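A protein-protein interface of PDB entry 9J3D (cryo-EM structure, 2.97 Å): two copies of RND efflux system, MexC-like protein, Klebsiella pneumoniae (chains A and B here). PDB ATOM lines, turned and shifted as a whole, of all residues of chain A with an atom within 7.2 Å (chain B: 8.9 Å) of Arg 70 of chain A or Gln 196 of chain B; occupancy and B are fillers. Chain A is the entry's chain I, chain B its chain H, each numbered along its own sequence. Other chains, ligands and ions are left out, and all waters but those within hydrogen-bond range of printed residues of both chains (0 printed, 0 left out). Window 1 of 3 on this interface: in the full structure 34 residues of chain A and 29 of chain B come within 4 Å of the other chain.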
ATOM      1  N   ARG A  68       4.654 -25.329  -7.670  1.00  0.00           N
ATOM      2  CA  ARG A  68       3.599 -24.387  -8.004  1.00  0.00           C
ATOM      3  C   ARG A  68       3.129 -23.671  -6.747  1.00  0.00           C
ATOM      4  O   ARG A  68       3.344 -24.144  -5.628  1.00  0.00           O
ATOM      5  CB  ARG A  68       2.406 -25.096  -8.655  1.00  0.00           C
ATOM      6  CG  ARG A  68       2.716 -25.776  -9.973  1.00  0.00           C
ATOM      7  CD  ARG A  68       1.462 -26.387 -10.574  1.00  0.00           C
ATOM      8  NE  ARG A  68       1.688 -26.890 -11.922  1.00  0.00           N
ATOM      9  CZ  ARG A  68       1.165 -26.357 -13.017  1.00  0.00           C
ATOM     10  NH1 ARG A  68       0.378 -25.296 -12.959  1.00  0.00           N
ATOM     11  NH2 ARG A  68       1.438 -26.902 -14.198  1.00  0.00           N
ATOM     12  N   ALA A  69       2.478 -22.528  -6.940  1.00  0.00           N
ATOM     13  CA  ALA A  69       1.947 -21.765  -5.818  1.00  0.00           C
ATOM     14  C   ALA A  69       0.589 -22.318  -5.408  1.00  0.00           C
ATOM     15  O   ALA A  69      -0.297 -22.492  -6.249  1.00  0.00           O
ATOM     16  CB  ALA A  69       1.836 -20.290  -6.190  1.00  0.00           C
ATOM     17  N   ARG A  70       0.424 -22.596  -4.114  1.00  0.00           N
ATOM     18  CA  ARG A  70      -0.843 -23.099  -3.606  1.00  0.00           C
ATOM     19  C   ARG A  70      -1.758 -21.995  -3.098  1.00  0.00           C
ATOM     20  O   ARG A  70      -2.958 -22.233  -2.928  1.00  0.00           O
ATOM     21  CB  ARG A  70      -0.606 -24.106  -2.476  1.00  0.00           C
ATOM     22  CG  ARG A  70       0.594 -25.013  -2.684  1.00  0.00           C
ATOM     23  CD  ARG A  70       0.183 -26.380  -3.194  1.00  0.00           C
ATOM     24  NE  ARG A  70      -0.998 -26.910  -2.529  1.00  0.00           N
ATOM     25  CZ  ARG A  70      -0.964 -27.660  -1.439  1.00  0.00           C
ATOM     26  NH1 ARG A  70       0.181 -27.974  -0.857  1.00  0.00           N
ATOM     27  NH2 ARG A  70      -2.105 -28.125  -0.939  1.00  0.00           N
ATOM     28  N   VAL A  71      -1.224 -20.802  -2.851  1.00  0.00           N
ATOM     29  CA  VAL A  71      -1.990 -19.692  -2.302  1.00  0.00           C
ATOM     30  C   VAL A  71      -1.692 -18.437  -3.106  1.00  0.00           C
ATOM     31  O   VAL A  71      -0.679 -18.351  -3.806  1.00  0.00           O
ATOM     32  CB  VAL A  71      -1.677 -19.463  -0.808  1.00  0.00           C
ATOM     33  CG1 VAL A  71      -2.158 -20.639   0.026  1.00  0.00           C
ATOM     34  CG2 VAL A  71      -0.188 -19.233  -0.608  1.00  0.00           C
ATOM     35  N   ALA A  72      -2.582 -17.456  -2.996  1.00  0.00           N
ATOM     36  CA  ALA A  72      -2.430 -16.209  -3.730  1.00  0.00           C
ATOM     37  C   ALA A  72      -1.612 -15.208  -2.928  1.00  0.00           C
ATOM     38  O   ALA A  72      -1.805 -15.051  -1.720  1.00  0.00           O
ATOM     39  CB  ALA A  72      -3.798 -15.618  -4.060  1.00  0.00           C
ATOM     40  N   ILE A  95       6.282 -16.299  -0.248  1.00  0.00           N
ATOM     41  CA  ILE A  95       5.098 -15.543  -0.634  1.00  0.00           C
ATOM     42  C   ILE A  95       4.644 -14.725   0.564  1.00  0.00           C
ATOM     43  O   ILE A  95       4.670 -15.208   1.701  1.00  0.00           O
ATOM     44  CB  ILE A  95       3.984 -16.480  -1.133  1.00  0.00           C
ATOM     45  CG1 ILE A  95       4.486 -17.324  -2.304  1.00  0.00           C
ATOM     46  CG2 ILE A  95       2.760 -15.686  -1.545  1.00  0.00           C
ATOM     47  CD1 ILE A  95       3.489 -18.347  -2.787  1.00  0.00           C
ATOM     48  N   PHE A 100      -2.779 -15.017   5.895  1.00  0.00           N
ATOM     49  CA  PHE A 100      -2.663 -16.281   6.612  1.00  0.00           C
ATOM     50  C   PHE A 100      -2.124 -16.076   8.020  1.00  0.00           C
ATOM     51  O   PHE A 100      -2.485 -16.817   8.940  1.00  0.00           O
ATOM     52  CB  PHE A 100      -1.789 -17.242   5.814  1.00  0.00           C
ATOM     53  CG  PHE A 100      -2.184 -17.340   4.373  1.00  0.00           C
ATOM     54  CD1 PHE A 100      -3.403 -17.887   4.017  1.00  0.00           C
ATOM     55  CD2 PHE A 100      -1.352 -16.866   3.377  1.00  0.00           C
ATOM     56  CE1 PHE A 100      -3.780 -17.972   2.695  1.00  0.00           C
ATOM     57  CE2 PHE A 100      -1.725 -16.948   2.051  1.00  0.00           C
ATOM     58  CZ  PHE A 100      -2.941 -17.500   1.713  1.00  0.00           C
ATOM     59  N   LEU A 168      -0.786 -25.047   8.873  1.00  0.00           N
ATOM     60  CA  LEU A 168      -0.402 -25.688   7.619  1.00  0.00           C
ATOM     61  C   LEU A 168      -0.724 -24.786   6.432  1.00  0.00           C
ATOM     62  O   LEU A 168       0.047 -24.706   5.468  1.00  0.00           O
ATOM     63  CB  LEU A 168      -1.078 -27.057   7.488  1.00  0.00           C
ATOM     64  CG  LEU A 168      -2.543 -27.221   7.080  1.00  0.00           C
ATOM     65  CD1 LEU A 168      -2.704 -27.305   5.570  1.00  0.00           C
ATOM     66  CD2 LEU A 168      -3.130 -28.452   7.746  1.00  0.00           C
ATOM     67  N   ASP A 169      -1.854 -24.077   6.497  1.00  0.00           N
ATOM     68  CA  ASP A 169      -2.174 -23.115   5.449  1.00  0.00           C
ATOM     69  C   ASP A 169      -1.086 -22.054   5.346  1.00  0.00           C
ATOM     70  O   ASP A 169      -0.652 -21.702   4.244  1.00  0.00           O
ATOM     71  CB  ASP A 169      -3.538 -22.482   5.735  1.00  0.00           C
ATOM     72  CG  ASP A 169      -3.939 -21.427   4.715  1.00  0.00           C
ATOM     73  OD1 ASP A 169      -3.250 -21.264   3.686  1.00  0.00           O
ATOM     74  OD2 ASP A 169      -4.963 -20.752   4.946  1.00  0.00           O
ATOM     75  N   TYR A 172       2.034 -23.329   3.794  1.00  0.00           N
ATOM     76  CA  TYR A 172       1.862 -23.453   2.350  1.00  0.00           C
ATOM     77  C   TYR A 172       2.234 -22.155   1.639  1.00  0.00           C
ATOM     78  O   TYR A 172       2.030 -22.027   0.428  1.00  0.00           O
ATOM     79  CB  TYR A 172       0.422 -23.855   2.029  1.00  0.00           C
ATOM     80  CG  TYR A 172       0.190 -25.348   2.009  1.00  0.00           C
ATOM     81  CD1 TYR A 172       1.179 -26.231   2.421  1.00  0.00           C
ATOM     82  CD2 TYR A 172      -1.035 -25.871   1.637  1.00  0.00           C
ATOM     83  CE1 TYR A 172       0.969 -27.599   2.414  1.00  0.00           C
ATOM     84  CE2 TYR A 172      -1.265 -27.226   1.669  1.00  0.00           C
ATOM     85  CZ  TYR A 172      -0.256 -28.091   2.034  1.00  0.00           C
ATOM     86  OH  TYR A 172      -0.477 -29.453   2.024  1.00  0.00           O
ATOM     87  N   ALA A 173       2.767 -21.183   2.381  1.00  0.00           N
ATOM     88  CA  ALA A 173       3.295 -19.954   1.799  1.00  0.00           C
ATOM     89  C   ALA A 173       4.815 -19.927   1.738  1.00  0.00           C
ATOM     90  O   ALA A 173       5.377 -19.200   0.913  1.00  0.00           O
ATOM     91  CB  ALA A 173       2.803 -18.733   2.582  1.00  0.00           C
ATOM     92  N   VAL A 175       7.266 -21.788   0.212  1.00  0.00           N
ATOM     93  CA  VAL A 175       7.256 -22.803  -0.835  1.00  0.00           C
ATOM     94  C   VAL A 175       8.524 -23.638  -0.700  1.00  0.00           C
ATOM     95  O   VAL A 175       9.612 -23.195  -1.073  1.00  0.00           O
ATOM     96  CB  VAL A 175       7.154 -22.168  -2.225  1.00  0.00           C
ATOM     97  CG1 VAL A 175       6.745 -23.207  -3.239  1.00  0.00           C
ATOM     98  CG2 VAL A 175       6.168 -21.016  -2.207  1.00  0.00           C
ATOM     99  N   VAL A 194       1.353 -14.399  -7.702  1.00  0.00           N
ATOM    100  CA  VAL A 194       1.194 -15.813  -8.006  1.00  0.00           C
ATOM    101  C   VAL A 194       0.055 -16.373  -7.166  1.00  0.00           C
ATOM    102  O   VAL A 194      -0.343 -15.800  -6.152  1.00  0.00           O
ATOM    103  CB  VAL A 194       2.488 -16.614  -7.756  1.00  0.00           C
ATOM    104  CG1 VAL A 194       3.635 -16.042  -8.572  1.00  0.00           C
ATOM    105  CG2 VAL A 194       2.827 -16.621  -6.277  1.00  0.00           C
ATOM    106  N   GLY A 195      -0.470 -17.511  -7.611  1.00  0.00           N
ATOM    107  CA  GLY A 195      -1.509 -18.197  -6.874  1.00  0.00           C
ATOM    108  C   GLY A 195      -2.901 -17.641  -7.043  1.00  0.00           C
ATOM    109  O   GLY A 195      -3.827 -18.126  -6.389  1.00  0.00           O
ATOM    110  N   GLY A 197      -6.192 -17.519  -8.843  1.00  0.00           N
ATOM    111  CA  GLY A 197      -6.949 -18.310  -9.790  1.00  0.00           C
ATOM    112  C   GLY A 197      -6.400 -19.709  -9.975  1.00  0.00           C
ATOM    113  O   GLY A 197      -7.009 -20.686  -9.529  1.00  0.00           O
ATOM    114  N   GLU A 198      -5.246 -19.818 -10.624  1.00  0.00           N
ATOM    115  CA  GLU A 198      -4.626 -21.102 -10.911  1.00  0.00           C
ATOM    116  C   GLU A 198      -3.312 -21.232 -10.155  1.00  0.00           C
ATOM    117  O   GLU A 198      -2.739 -20.242  -9.692  1.00  0.00           O
ATOM    118  CB  GLU A 198      -4.377 -21.275 -12.415  1.00  0.00           C
ATOM    119  CG  GLU A 198      -3.184 -20.497 -12.965  1.00  0.00           C
ATOM    120  CD  GLU A 198      -3.337 -18.991 -12.850  1.00  0.00           C
ATOM    121  OE1 GLU A 198      -4.478 -18.514 -12.674  1.00  0.00           O
ATOM    122  OE2 GLU A 198      -2.312 -18.282 -12.938  1.00  0.00           O
ATOM    123  N   ALA A 199      -2.839 -22.471 -10.034  1.00  0.00           N
ATOM    124  CA  ALA A 199      -1.559 -22.735  -9.393  1.00  0.00           C
ATOM    125  C   ALA A 199      -0.420 -22.306 -10.307  1.00  0.00           C
ATOM    126  O   ALA A 199      -0.025 -23.053 -11.208  1.00  0.00           O
ATOM    127  CB  ALA A 199      -1.431 -24.214  -9.035  1.00  0.00           C
ATOM    128  N   THR A 200       0.106 -21.105 -10.086  1.00  0.00           N
ATOM    129  CA  THR A 200       1.166 -20.588 -10.939  1.00  0.00           C
ATOM    130  C   THR A 200       2.418 -21.441 -10.805  1.00  0.00           C
ATOM    131  O   THR A 200       2.906 -21.683  -9.699  1.00  0.00           O
ATOM    132  CB  THR A 200       1.475 -19.136 -10.576  1.00  0.00           C
ATOM    133  OG1 THR A 200       0.252 -18.400 -10.457  1.00  0.00           O
ATOM    134  CG2 THR A 200       2.343 -18.494 -11.645  1.00  0.00           C
ATOM    135  N   LEU A 202       5.976 -22.189 -10.418  1.00  0.00           N
ATOM    136  CA  LEU A 202       7.123 -21.446  -9.916  1.00  0.00           C
ATOM    137  C   LEU A 202       8.449 -22.003 -10.408  1.00  0.00           C
ATOM    138  O   LEU A 202       9.316 -21.235 -10.832  1.00  0.00           O
ATOM    139  CB  LEU A 202       7.114 -21.429  -8.386  1.00  0.00           C
ATOM    140  CG  LEU A 202       5.827 -20.933  -7.726  1.00  0.00           C
ATOM    141  CD1 LEU A 202       5.963 -20.949  -6.213  1.00  0.00           C
ATOM    142  CD2 LEU A 202       5.476 -19.544  -8.222  1.00  0.00           C
ATOM    143  N   ALA B  69      -6.913 -37.910  -8.944  1.00  0.00           N
ATOM    144  CA  ALA B  69      -6.844 -37.365  -7.595  1.00  0.00           C
ATOM    145  C   ALA B  69      -8.063 -36.496  -7.322  1.00  0.00           C
ATOM    146  O   ALA B  69      -8.443 -35.667  -8.156  1.00  0.00           O
ATOM    147  CB  ALA B  69      -5.562 -36.559  -7.417  1.00  0.00           C
ATOM    148  N   ARG B  70      -8.675 -36.680  -6.153  1.00  0.00           N
ATOM    149  CA  ARG B  70      -9.830 -35.884  -5.763  1.00  0.00           C
ATOM    150  C   ARG B  70      -9.485 -34.760  -4.800  1.00  0.00           C
ATOM    151  O   ARG B  70     -10.250 -33.794  -4.702  1.00  0.00           O
ATOM    152  CB  ARG B  70     -10.897 -36.766  -5.113  1.00  0.00           C
ATOM    153  CG  ARG B  70     -11.355 -37.938  -5.949  1.00  0.00           C
ATOM    154  CD  ARG B  70     -12.499 -38.641  -5.250  1.00  0.00           C
ATOM    155  NE  ARG B  70     -12.831 -39.920  -5.861  1.00  0.00           N
ATOM    156  CZ  ARG B  70     -13.884 -40.650  -5.527  1.00  0.00           C
ATOM    157  NH1 ARG B  70     -14.747 -40.242  -4.612  1.00  0.00           N
ATOM    158  NH2 ARG B  70     -14.078 -41.820  -6.127  1.00  0.00           N
ATOM    159  N   VAL B  71      -8.366 -34.859  -4.089  1.00  0.00           N
ATOM    160  CA  VAL B  71      -7.989 -33.878  -3.081  1.00  0.00           C
ATOM    161  C   VAL B  71      -6.604 -33.339  -3.400  1.00  0.00           C
ATOM    162  O   VAL B  71      -5.722 -34.067  -3.867  1.00  0.00           O
ATOM    163  CB  VAL B  71      -8.031 -34.475  -1.658  1.00  0.00           C
ATOM    164  CG1 VAL B  71      -9.452 -34.854  -1.289  1.00  0.00           C
ATOM    165  CG2 VAL B  71      -7.117 -35.681  -1.557  1.00  0.00           C
ATOM    166  N   ALA B  72      -6.420 -32.046  -3.156  1.00  0.00           N
ATOM    167  CA  ALA B  72      -5.165 -31.382  -3.477  1.00  0.00           C
ATOM    168  C   ALA B  72      -4.097 -31.703  -2.440  1.00  0.00           C
ATOM    169  O   ALA B  72      -4.364 -31.721  -1.235  1.00  0.00           O
ATOM    170  CB  ALA B  72      -5.371 -29.871  -3.564  1.00  0.00           C
ATOM    171  N   GLY B  73      -2.883 -31.948  -2.914  1.00  0.00           N
ATOM    172  CA  GLY B  73      -1.781 -32.244  -2.022  1.00  0.00           C
ATOM    173  C   GLY B  73      -0.585 -32.757  -2.791  1.00  0.00           C
ATOM    174  O   GLY B  73      -0.606 -32.878  -4.019  1.00  0.00           O
ATOM    175  N   ILE B  74       0.465 -33.058  -2.036  1.00  0.00           N
ATOM    176  CA  ILE B  74       1.708 -33.562  -2.608  1.00  0.00           C
ATOM    177  C   ILE B  74       1.668 -35.083  -2.617  1.00  0.00           C
ATOM    178  O   ILE B  74       1.323 -35.712  -1.611  1.00  0.00           O
ATOM    179  CB  ILE B  74       2.918 -33.044  -1.814  1.00  0.00           C
ATOM    180  CG1 ILE B  74       3.210 -31.583  -2.161  1.00  0.00           C
ATOM    181  CG2 ILE B  74       4.142 -33.903  -2.072  1.00  0.00           C
ATOM    182  CD1 ILE B  74       2.997 -31.237  -3.612  1.00  0.00           C
ATOM    183  N   VAL B  75       2.019 -35.679  -3.755  1.00  0.00           N
ATOM    184  CA  VAL B  75       2.072 -37.133  -3.865  1.00  0.00           C
ATOM    185  C   VAL B  75       3.332 -37.616  -3.154  1.00  0.00           C
ATOM    186  O   VAL B  75       4.438 -37.503  -3.690  1.00  0.00           O
ATOM    187  CB  VAL B  75       2.051 -37.586  -5.328  1.00  0.00           C
ATOM    188  CG1 VAL B  75       2.136 -39.099  -5.414  1.00  0.00           C
ATOM    189  CG2 VAL B  75       0.803 -37.080  -6.020  1.00  0.00           C
ATOM    190  N   ILE B  95      -1.287 -39.479  -1.018  1.00  0.00           N
ATOM    191  CA  ILE B  95      -1.174 -38.027  -0.966  1.00  0.00           C
ATOM    192  C   ILE B  95      -1.149 -37.611   0.494  1.00  0.00           C
ATOM    193  O   ILE B  95      -1.894 -38.156   1.315  1.00  0.00           O
ATOM    194  CB  ILE B  95      -2.336 -37.357  -1.722  1.00  0.00           C
ATOM    195  CG1 ILE B  95      -2.438 -37.908  -3.142  1.00  0.00           C
ATOM    196  CG2 ILE B  95      -2.156 -35.856  -1.754  1.00  0.00           C
ATOM    197  CD1 ILE B  95      -3.668 -37.447  -3.887  1.00  0.00           C
ATOM    198  N   ASP B  96      -0.285 -36.658   0.827  1.00  0.00           N
ATOM    199  CA  ASP B  96      -0.104 -36.287   2.223  1.00  0.00           C
ATOM    200  C   ASP B  96      -1.367 -35.627   2.770  1.00  0.00           C
ATOM    201  O   ASP B  96      -1.804 -34.593   2.257  1.00  0.00           O
ATOM    202  CB  ASP B  96       1.090 -35.342   2.378  1.00  0.00           C
ATOM    203  CG  ASP B  96       0.923 -34.047   1.603  1.00  0.00           C
ATOM    204  OD1 ASP B  96       0.247 -34.061   0.553  1.00  0.00           O
ATOM    205  OD2 ASP B  96       1.463 -33.013   2.048  1.00  0.00           O
ATOM    206  N   ALA B  98      -2.471 -33.253   5.130  1.00  0.00           N
ATOM    207  CA  ALA B  98      -2.304 -32.225   6.147  1.00  0.00           C
ATOM    208  C   ALA B  98      -3.659 -31.710   6.628  1.00  0.00           C
ATOM    209  O   ALA B  98      -3.909 -31.693   7.839  1.00  0.00           O
ATOM    210  CB  ALA B  98      -1.425 -31.083   5.632  1.00  0.00           C
ATOM    211  N   PRO B  99      -4.564 -31.290   5.731  1.00  0.00           N
ATOM    212  CA  PRO B  99      -5.828 -30.715   6.217  1.00  0.00           C
ATOM    213  C   PRO B  99      -6.871 -31.754   6.578  1.00  0.00           C
ATOM    214  O   PRO B  99      -7.657 -31.540   7.510  1.00  0.00           O
ATOM    215  CB  PRO B  99      -6.288 -29.842   5.036  1.00  0.00           C
ATOM    216  CG  PRO B  99      -5.122 -29.811   4.076  1.00  0.00           C
ATOM    217  CD  PRO B  99      -4.465 -31.126   4.273  1.00  0.00           C
ATOM    218  N   PHE B 100      -6.914 -32.871   5.852  1.00  0.00           N
ATOM    219  CA  PHE B 100      -7.969 -33.855   6.068  1.00  0.00           C
ATOM    220  C   PHE B 100      -7.815 -34.544   7.417  1.00  0.00           C
ATOM    221  O   PHE B 100      -8.812 -34.854   8.080  1.00  0.00           O
ATOM    222  CB  PHE B 100      -7.969 -34.865   4.925  1.00  0.00           C
ATOM    223  CG  PHE B 100      -7.462 -34.301   3.628  1.00  0.00           C
ATOM    224  CD1 PHE B 100      -8.196 -33.353   2.937  1.00  0.00           C
ATOM    225  CD2 PHE B 100      -6.250 -34.709   3.106  1.00  0.00           C
ATOM    226  CE1 PHE B 100      -7.731 -32.830   1.749  1.00  0.00           C
ATOM    227  CE2 PHE B 100      -5.781 -34.189   1.918  1.00  0.00           C
ATOM    228  CZ  PHE B 100      -6.521 -33.248   1.242  1.00  0.00           C
ATOM    229  N   ALA B 192       5.054 -34.550  -7.016  1.00  0.00           N
ATOM    230  CA  ALA B 192       4.321 -33.625  -7.867  1.00  0.00           C
ATOM    231  C   ALA B 192       3.022 -33.192  -7.200  1.00  0.00           C
ATOM    232  O   ALA B 192       2.389 -33.962  -6.472  1.00  0.00           O
ATOM    233  CB  ALA B 192       4.025 -34.269  -9.219  1.00  0.00           C
ATOM    234  N   LEU B 193       2.622 -31.947  -7.453  1.00  0.00           N
ATOM    235  CA  LEU B 193       1.377 -31.424  -6.907  1.00  0.00           C
ATOM    236  C   LEU B 193       0.204 -31.836  -7.783  1.00  0.00           C
ATOM    237  O   LEU B 193       0.223 -31.627  -9.000  1.00  0.00           O
ATOM    238  CB  LEU B 193       1.437 -29.903  -6.796  1.00  0.00           C
ATOM    239  CG  LEU B 193       0.128 -29.234  -6.372  1.00  0.00           C
ATOM    240  CD1 LEU B 193      -0.220 -29.592  -4.940  1.00  0.00           C
ATOM    241  CD2 LEU B 193       0.203 -27.729  -6.552  1.00  0.00           C
ATOM    242  N   VAL B 194      -0.821 -32.417  -7.162  1.00  0.00           N
ATOM    243  CA  VAL B 194      -2.012 -32.874  -7.862  1.00  0.00           C
ATOM    244  C   VAL B 194      -3.240 -32.373  -7.115  1.00  0.00           C
ATOM    245  O   VAL B 194      -3.170 -31.976  -5.953  1.00  0.00           O
ATOM    246  CB  VAL B 194      -2.064 -34.409  -7.997  1.00  0.00           C
ATOM    247  CG1 VAL B 194      -0.834 -34.925  -8.720  1.00  0.00           C
ATOM    248  CG2 VAL B 194      -2.198 -35.051  -6.631  1.00  0.00           C
ATOM    249  N   GLY B 195      -4.374 -32.392  -7.809  1.00  0.00           N
ATOM    250  CA  GLY B 195      -5.649 -32.095  -7.188  1.00  0.00           C
ATOM    251  C   GLY B 195      -6.010 -30.633  -7.071  1.00  0.00           C
ATOM    252  O   GLY B 195      -7.064 -30.319  -6.512  1.00  0.00           O
ATOM    253  N   GLN B 196      -5.181 -29.726  -7.577  1.00  0.00           N
ATOM    254  CA  GLN B 196      -5.485 -28.302  -7.530  1.00  0.00           C
ATOM    255  C   GLN B 196      -6.196 -27.894  -8.812  1.00  0.00           C
ATOM    256  O   GLN B 196      -5.667 -28.090  -9.911  1.00  0.00           O
ATOM    257  CB  GLN B 196      -4.215 -27.475  -7.335  1.00  0.00           C
ATOM    258  CG  GLN B 196      -3.732 -27.424  -5.901  1.00  0.00           C
ATOM    259  CD  GLN B 196      -3.231 -26.049  -5.511  1.00  0.00           C
ATOM    260  OE1 GLN B 196      -2.991 -25.199  -6.366  1.00  0.00           O
ATOM    261  NE2 GLN B 196      -3.083 -25.819  -4.213  1.00  0.00           N
ATOM    262  N   GLY B 197      -7.388 -27.324  -8.669  1.00  0.00           N
ATOM    263  CA  GLY B 197      -8.161 -26.892  -9.816  1.00  0.00           C
ATOM    264  C   GLY B 197      -8.952 -28.012 -10.455  1.00  0.00           C
ATOM    265  O   GLY B 197     -10.178 -28.070 -10.325  1.00  0.00           O
ATOM    266  N   GLU B 198      -8.260 -28.911 -11.147  1.00  0.00           N
ATOM    267  CA  GLU B 198      -8.886 -30.024 -11.841  1.00  0.00           C
ATOM    268  C   GLU B 198      -8.484 -31.341 -11.194  1.00  0.00           C
ATOM    269  O   GLU B 198      -7.475 -31.423 -10.488  1.00  0.00           O
ATOM    270  CB  GLU B 198      -8.497 -30.037 -13.323  1.00  0.00           C
ATOM    271  CG  GLU B 198      -7.266 -30.879 -13.653  1.00  0.00           C
ATOM    272  CD  GLU B 198      -5.967 -30.291 -13.126  1.00  0.00           C
ATOM    273  OE1 GLU B 198      -4.905 -30.913 -13.342  1.00  0.00           O
ATOM    274  OE2 GLU B 198      -5.994 -29.203 -12.513  1.00  0.00           O
ATOM    275  N   ALA B 199      -9.287 -32.375 -11.438  1.00  0.00           N
ATOM    276  CA  ALA B 199      -8.951 -33.712 -10.967  1.00  0.00           C
ATOM    277  C   ALA B 199      -7.801 -34.270 -11.791  1.00  0.00           C
ATOM    278  O   ALA B 199      -8.009 -34.760 -12.906  1.00  0.00           O
ATOM    279  CB  ALA B 199     -10.169 -34.634 -11.042  1.00  0.00           C
ATOM    280  N   THR B 200      -6.585 -34.196 -11.255  1.00  0.00           N
ATOM    281  CA  THR B 200      -5.409 -34.619 -12.001  1.00  0.00           C
ATOM    282  C   THR B 200      -5.454 -36.115 -12.276  1.00  0.00           C
ATOM    283  O   THR B 200      -5.745 -36.915 -11.383  1.00  0.00           O
ATOM    284  CB  THR B 200      -4.140 -34.269 -11.224  1.00  0.00           C
ATOM    285  OG1 THR B 200      -4.236 -32.926 -10.736  1.00  0.00           O
ATOM    286  CG2 THR B 200      -2.920 -34.392 -12.116  1.00  0.00           C
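NE2 of Gln 196 of chain B sits close to NE of Arg 70 of chain A (2.9 Å).
Printed residues of chain B within 4 Å of Ala 69 of chain A: Gln 196 (3.8 Å). No residue of chain B comes within 4 Å of Val 71 of chain A. Of the printed residues of chain B, Leu 168 of chain A touches Ala 98 (3.3 Å) and Pro 99 (3.8 Å). Of the printed residues of chain B, Ala 199 of chain A touches Gln 196 (3.2 Å). Printed residues of chain A within 4 Å of Ala 98 of chain B: Leu 168. Of the printed residues of chain A, Pro 99 of chain B touches Leu 168. Printed residues of chain A within 4 Å of Leu 193 of chain B: Arg 70 (3.6 Å). Gln 196 of chain B touches just these residues of chain A: Ala 69 (3.8 Å), Arg 70 (2.9 Å) and Ala 199 (3.2 Å). The nearest printed residue of chain B that does not touch Arg 70 of chain A is Ala 72 of chain B (4.3 Å).
Ala 69 of chain A touches Gln 196 of chain B (O to OE1, 3.8 Å). Arg 70 of chain A touches Leu 193 of chain B (CD to CD2, 3.6 Å). CD2 of Leu 168 of chain A touches O of Ala 98 of chain B, 3.3 Å away. Leu 168 of chain A touches Pro 99 of chain B. OE1 of Gln 196 of chain B touches CB of Ala 199 of chain A (3.2 Å).
Positions printed for both chains: 69, 70, 71, 72, 95, 100, 194, 195, 197, 198, 199 and 200. Of the 6 pairs that touch across the chains among the printed residues, none has its exchanged pair printed and touching as well.
The guanidinium group (NH1) of Arg 68 of chain A lies within hydrogen-bond range of the backbone carbonyl oxygen (O) of Ala 199 of chain A, 2.9 Å away. N of Ala 69 of chain A sits at hydrogen-bond distance from O of Thr 200 of chain A, 2.9 Å away. NH1 of Arg 70 of chain A sits close to OH of Tyr 172 of chain A, 3.3 Å away.
Hydrophobic or aromatic side chains of chain A within 4 Å of the printed part of chain B: Leu 168 and Ala 199. Among the printed residues, no Asp or Glu carboxylate lies within 4 Å of a Lys or Arg side-chain nitrogen of the other chain.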
